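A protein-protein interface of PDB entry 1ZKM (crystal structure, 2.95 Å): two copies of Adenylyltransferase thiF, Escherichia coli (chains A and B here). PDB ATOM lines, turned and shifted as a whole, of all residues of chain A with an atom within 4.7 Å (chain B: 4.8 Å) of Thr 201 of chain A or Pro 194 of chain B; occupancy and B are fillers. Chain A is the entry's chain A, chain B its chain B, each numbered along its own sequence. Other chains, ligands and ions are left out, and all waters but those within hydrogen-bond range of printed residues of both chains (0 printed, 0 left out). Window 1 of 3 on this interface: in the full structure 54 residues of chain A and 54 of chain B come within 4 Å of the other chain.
CE2 of Tyr 48 of chain A touches O of Gly 193 of chain B (3.6 Å).
Tyr 48 of chain A touches Pro 194 of chain B.
Gly 197 of chain B touches Tyr 48 of chain A.
Val 198 of chain B touches Val 198 of chain A (O to CG2, 3.9 Å).
Thr 201 of chain B touches Val 198 of chain A (CG2 to CG2, 3.6 Å).
Pro 194 of chain B touches Thr 201 of chain A (O to CG2, 3.6 Å).
Thr 201 of chain A touches Val 198 of chain B.
CG2 of Val 198 of chain B touches CD2 of Leu 202 of chain A, at 3.6 Å.
Leu 205 of chain A touches Pro 194 of chain B.
Ile 208 of chain A touches Pro 194 of chain B.
OG1 of Thr 201 of chain A sits at hydrogen-bond distance from O of Gly 197 of chain A (3.2 Å).
The backbone carbonyl oxygen (O) of Gly 197 of chain B lies within hydrogen-bond range of the side-chain hydroxyl (OG1) of Thr 201 of chain B, 3.1 Å away.
Val 198 of chain B touches its own counterpart, Val 198 of chain A.
Val 198 of chain A touches Thr 201 of chain B, and with the chains exchanged Thr 201 of chain A touches Val 198 of chain B.
Positions printed for both chains: 197, 198 and 201.
Of the 10 pairs that touch across the chains among the printed residues, 3 have their exchanged pair printed and touching as well.
Of chain A, only Tyr 48 (3.5 Å), Thr 201 (3.6 Å), Leu 205 (3.5 Å) and Ile 208 (3.9 Å) come within 4 Å of Pro 194 of chain B.
Of the printed residues of chain A, Thr 201 of chain B touches Val 198.
Printed residues of chain A within 4 Å of Val 198 of chain B: Val 198 (3.9 Å), Thr 201 (3.7 Å) and Leu 202 (3.6 Å).
Printed residues of chain B within 4 Å of Tyr 48 of chain A: Gly 193 (3.6 Å), Pro 194 (3.5 Å) and Gly 197 (3.1 Å).
Pro 44 of chain A touches none of the printed residues of chain B.
Val 196 of chain B touches none of the printed residues of chain A.
The nearest residue of chain B that does not touch Thr 201 of chain A is Gly 197 of chain B (4.4 Å).
The nearest residue of chain A that does not touch Pro 194 of chain B is Ala 204 of chain A (4.1 Å).
Of the 8 printed residues of chain B, 5 touch a printed residue of chain A.
Hydrophobic or aromatic side chains of chain B within 4 Å of the printed part of chain A: Pro 194 and Val 198.
Hydrophobic or aromatic side chains of chain A within 4 Å of the printed part of chain B: Tyr 48, Val 198, Leu 202, Leu 205 and Ile 208.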
ATOM      1  N   PRO A  44       4.016  17.279  11.610  1.00  0.00           N
ATOM      2  CA  PRO A  44       3.590  15.952  12.036  1.00  0.00           C
ATOM      3  C   PRO A  44       2.154  15.720  11.588  1.00  0.00           C
ATOM      4  O   PRO A  44       1.647  14.616  11.670  1.00  0.00           O
ATOM      5  CB  PRO A  44       3.728  16.029  13.548  1.00  0.00           C
ATOM      6  CG  PRO A  44       3.215  17.394  13.807  1.00  0.00           C
ATOM      7  CD  PRO A  44       3.871  18.247  12.709  1.00  0.00           C
ATOM      8  N   TYR A  48       1.537  12.105   9.489  1.00  0.00           N
ATOM      9  CA  TYR A  48       0.544  11.113   9.866  1.00  0.00           C
ATOM     10  C   TYR A  48      -0.590  10.964   8.867  1.00  0.00           C
ATOM     11  O   TYR A  48      -1.195   9.889   8.780  1.00  0.00           O
ATOM     12  CB  TYR A  48      -0.055  11.431  11.228  1.00  0.00           C
ATOM     13  CG  TYR A  48       0.813  11.038  12.378  1.00  0.00           C
ATOM     14  CD1 TYR A  48       1.678  11.959  12.985  1.00  0.00           C
ATOM     15  CD2 TYR A  48       0.793   9.736  12.856  1.00  0.00           C
ATOM     16  CE1 TYR A  48       2.502  11.584  14.045  1.00  0.00           C
ATOM     17  CE2 TYR A  48       1.616   9.346  13.912  1.00  0.00           C
ATOM     18  CZ  TYR A  48       2.469  10.272  14.501  1.00  0.00           C
ATOM     19  OH  TYR A  48       3.294   9.849  15.514  1.00  0.00           O
ATOM     20  N   GLY A 197       3.905  19.779  18.812  1.00  0.00           N
ATOM     21  CA  GLY A 197       3.785  18.489  18.153  1.00  0.00           C
ATOM     22  C   GLY A 197       2.444  17.827  18.405  1.00  0.00           C
ATOM     23  O   GLY A 197       1.677  17.587  17.476  1.00  0.00           O
ATOM     24  N   VAL A 198       2.153  17.520  19.663  1.00  0.00           N
ATOM     25  CA  VAL A 198       0.883  16.906  20.017  1.00  0.00           C
ATOM     26  C   VAL A 198      -0.290  17.668  19.382  1.00  0.00           C
ATOM     27  O   VAL A 198      -1.285  17.080  18.965  1.00  0.00           O
ATOM     28  CB  VAL A 198       0.721  16.871  21.552  1.00  0.00           C
ATOM     29  CG1 VAL A 198      -0.740  16.959  21.942  1.00  0.00           C
ATOM     30  CG2 VAL A 198       1.310  15.590  22.085  1.00  0.00           C
ATOM     31  N   MET A 199      -0.172  18.984  19.305  1.00  0.00           N
ATOM     32  CA  MET A 199      -1.241  19.763  18.725  1.00  0.00           C
ATOM     33  C   MET A 199      -1.507  19.429  17.267  1.00  0.00           C
ATOM     34  O   MET A 199      -2.657  19.196  16.884  1.00  0.00           O
ATOM     35  CB  MET A 199      -0.950  21.253  18.882  1.00  0.00           C
ATOM     36  CG  MET A 199      -1.066  21.729  20.323  1.00  0.00           C
ATOM     37  SD  MET A 199      -2.626  21.217  21.074  1.00  0.00           S
ATOM     38  CE  MET A 199      -2.033  19.982  22.141  1.00  0.00           C
ATOM     39  N   GLY A 200      -0.449  19.407  16.458  1.00  0.00           N
ATOM     40  CA  GLY A 200      -0.597  19.095  15.045  1.00  0.00           C
ATOM     41  C   GLY A 200      -1.034  17.657  14.843  1.00  0.00           C
ATOM     42  O   GLY A 200      -1.940  17.362  14.062  1.00  0.00           O
ATOM     43  N   THR A 201      -0.384  16.752  15.559  1.00  0.00           N
ATOM     44  CA  THR A 201      -0.712  15.350  15.459  1.00  0.00           C
ATOM     45  C   THR A 201      -2.208  15.207  15.667  1.00  0.00           C
ATOM     46  O   THR A 201      -2.869  14.473  14.938  1.00  0.00           O
ATOM     47  CB  THR A 201       0.065  14.541  16.510  1.00  0.00           C
ATOM     48  OG1 THR A 201       1.471  14.620  16.222  1.00  0.00           O
ATOM     49  CG2 THR A 201      -0.379  13.079  16.507  1.00  0.00           C
ATOM     50  N   LEU A 202      -2.752  15.924  16.647  1.00  0.00           N
ATOM     51  CA  LEU A 202      -4.188  15.865  16.912  1.00  0.00           C
ATOM     52  C   LEU A 202      -4.974  16.492  15.771  1.00  0.00           C
ATOM     53  O   LEU A 202      -6.083  16.069  15.491  1.00  0.00           O
ATOM     54  CB  LEU A 202      -4.547  16.555  18.234  1.00  0.00           C
ATOM     55  CG  LEU A 202      -4.281  15.787  19.534  1.00  0.00           C
ATOM     56  CD1 LEU A 202      -4.654  16.660  20.713  1.00  0.00           C
ATOM     57  CD2 LEU A 202      -5.089  14.502  19.566  1.00  0.00           C
ATOM     58  N   GLN A 203      -4.422  17.497  15.104  1.00  0.00           N
ATOM     59  CA  GLN A 203      -5.156  18.079  13.981  1.00  0.00           C
ATOM     60  C   GLN A 203      -5.390  17.009  12.913  1.00  0.00           C
ATOM     61  O   GLN A 203      -6.373  17.060  12.182  1.00  0.00           O
ATOM     62  CB  GLN A 203      -4.383  19.216  13.320  1.00  0.00           C
ATOM     63  CG  GLN A 203      -4.252  20.476  14.114  1.00  0.00           C
ATOM     64  CD  GLN A 203      -3.396  21.483  13.391  1.00  0.00           C
ATOM     65  OE1 GLN A 203      -3.853  22.158  12.472  1.00  0.00           O
ATOM     66  NE2 GLN A 203      -2.131  21.570  13.784  1.00  0.00           N
ATOM     67  N   ALA A 204      -4.470  16.051  12.817  1.00  0.00           N
ATOM     68  CA  ALA A 204      -4.566  14.986  11.831  1.00  0.00           C
ATOM     69  C   ALA A 204      -5.568  13.938  12.266  1.00  0.00           C
ATOM     70  O   ALA A 204      -6.343  13.434  11.451  1.00  0.00           O
ATOM     71  CB  ALA A 204      -3.203  14.359  11.608  1.00  0.00           C
ATOM     72  N   LEU A 205      -5.550  13.591  13.545  1.00  0.00           N
ATOM     73  CA  LEU A 205      -6.515  12.610  14.051  1.00  0.00           C
ATOM     74  C   LEU A 205      -7.923  13.128  13.781  1.00  0.00           C
ATOM     75  O   LEU A 205      -8.832  12.365  13.471  1.00  0.00           O
ATOM     76  CB  LEU A 205      -6.354  12.393  15.563  1.00  0.00           C
ATOM     77  CG  LEU A 205      -7.567  11.759  16.244  1.00  0.00           C
ATOM     78  CD1 LEU A 205      -7.848  10.409  15.615  1.00  0.00           C
ATOM     79  CD2 LEU A 205      -7.303  11.590  17.726  1.00  0.00           C
ATOM     80  N   ILE A 208      -8.678  12.717   9.982  1.00  0.00           N
ATOM     81  CA  ILE A 208      -9.026  11.334   9.663  1.00  0.00           C
ATOM     82  C   ILE A 208     -10.471  11.074  10.047  1.00  0.00           C
ATOM     83  O   ILE A 208     -11.292  10.726   9.204  1.00  0.00           O
ATOM     84  CB  ILE A 208      -8.175  10.320  10.445  1.00  0.00           C
ATOM     85  CG1 ILE A 208      -6.747  10.301   9.897  1.00  0.00           C
ATOM     86  CG2 ILE A 208      -8.849   8.947  10.416  1.00  0.00           C
ATOM     87  CD1 ILE A 208      -5.832   9.395  10.678  1.00  0.00           C
ATOM     88  N   VAL B 192      -4.813   3.580  15.313  1.00  0.00           N
ATOM     89  CA  VAL B 192      -4.891   4.807  14.534  1.00  0.00           C
ATOM     90  C   VAL B 192      -3.516   5.473  14.616  1.00  0.00           C
ATOM     91  O   VAL B 192      -2.886   5.484  15.678  1.00  0.00           O
ATOM     92  CB  VAL B 192      -5.933   5.766  15.115  1.00  0.00           C
ATOM     93  CG1 VAL B 192      -6.015   7.011  14.246  1.00  0.00           C
ATOM     94  CG2 VAL B 192      -7.287   5.072  15.223  1.00  0.00           C
ATOM     95  N   GLY B 193      -3.042   6.024  13.505  1.00  0.00           N
ATOM     96  CA  GLY B 193      -1.734   6.652  13.520  1.00  0.00           C
ATOM     97  C   GLY B 193      -1.564   7.655  14.651  1.00  0.00           C
ATOM     98  O   GLY B 193      -0.866   7.407  15.639  1.00  0.00           O
ATOM     99  N   PRO B 194      -2.203   8.818  14.516  1.00  0.00           N
ATOM    100  CA  PRO B 194      -2.146   9.886  15.504  1.00  0.00           C
ATOM    101  C   PRO B 194      -2.338   9.466  16.959  1.00  0.00           C
ATOM    102  O   PRO B 194      -1.725  10.038  17.849  1.00  0.00           O
ATOM    103  CB  PRO B 194      -3.223  10.836  15.010  1.00  0.00           C
ATOM    104  CG  PRO B 194      -3.041  10.740  13.507  1.00  0.00           C
ATOM    105  CD  PRO B 194      -2.950   9.252  13.319  1.00  0.00           C
ATOM    106  N   VAL B 195      -3.168   8.476  17.230  1.00  0.00           N
ATOM    107  CA  VAL B 195      -3.354   8.108  18.627  1.00  0.00           C
ATOM    108  C   VAL B 195      -2.083   7.608  19.309  1.00  0.00           C
ATOM    109  O   VAL B 195      -1.823   7.986  20.450  1.00  0.00           O
ATOM    110  CB  VAL B 195      -4.489   7.086  18.797  1.00  0.00           C
ATOM    111  CG1 VAL B 195      -4.691   6.760  20.264  1.00  0.00           C
ATOM    112  CG2 VAL B 195      -5.764   7.660  18.219  1.00  0.00           C
ATOM    113  N   VAL B 196      -1.285   6.768  18.648  1.00  0.00           N
ATOM    114  CA  VAL B 196      -0.028   6.313  19.263  1.00  0.00           C
ATOM    115  C   VAL B 196       0.906   7.507  19.304  1.00  0.00           C
ATOM    116  O   VAL B 196       1.632   7.706  20.275  1.00  0.00           O
ATOM    117  CB  VAL B 196       0.728   5.250  18.446  1.00  0.00           C
ATOM    118  CG1 VAL B 196       0.686   3.925  19.165  1.00  0.00           C
ATOM    119  CG2 VAL B 196       0.185   5.178  17.028  1.00  0.00           C
ATOM    120  N   GLY B 197       0.895   8.274  18.217  1.00  0.00           N
ATOM    121  CA  GLY B 197       1.730   9.454  18.126  1.00  0.00           C
ATOM    122  C   GLY B 197       1.572  10.352  19.338  1.00  0.00           C
ATOM    123  O   GLY B 197       2.539  10.617  20.052  1.00  0.00           O
ATOM    124  N   VAL B 198       0.354  10.820  19.575  1.00  0.00           N
ATOM    125  CA  VAL B 198       0.095  11.675  20.713  1.00  0.00           C
ATOM    126  C   VAL B 198       0.735  11.069  21.955  1.00  0.00           C
ATOM    127  O   VAL B 198       1.472  11.736  22.677  1.00  0.00           O
ATOM    128  CB  VAL B 198      -1.406  11.834  20.939  1.00  0.00           C
ATOM    129  CG1 VAL B 198      -1.666  12.460  22.293  1.00  0.00           C
ATOM    130  CG2 VAL B 198      -1.995  12.698  19.846  1.00  0.00           C
ATOM    131  N   THR B 201       4.639  11.296  21.618  1.00  0.00           N
ATOM    132  CA  THR B 201       5.071  12.675  21.734  1.00  0.00           C
ATOM    133  C   THR B 201       4.949  13.078  23.211  1.00  0.00           C
ATOM    134  O   THR B 201       5.866  13.673  23.786  1.00  0.00           O
ATOM    135  CB  THR B 201       4.196  13.587  20.852  1.00  0.00           C
ATOM    136  OG1 THR B 201       4.283  13.156  19.488  1.00  0.00           O
ATOM    137  CG2 THR B 201       4.660  15.022  20.944  1.00  0.00           C
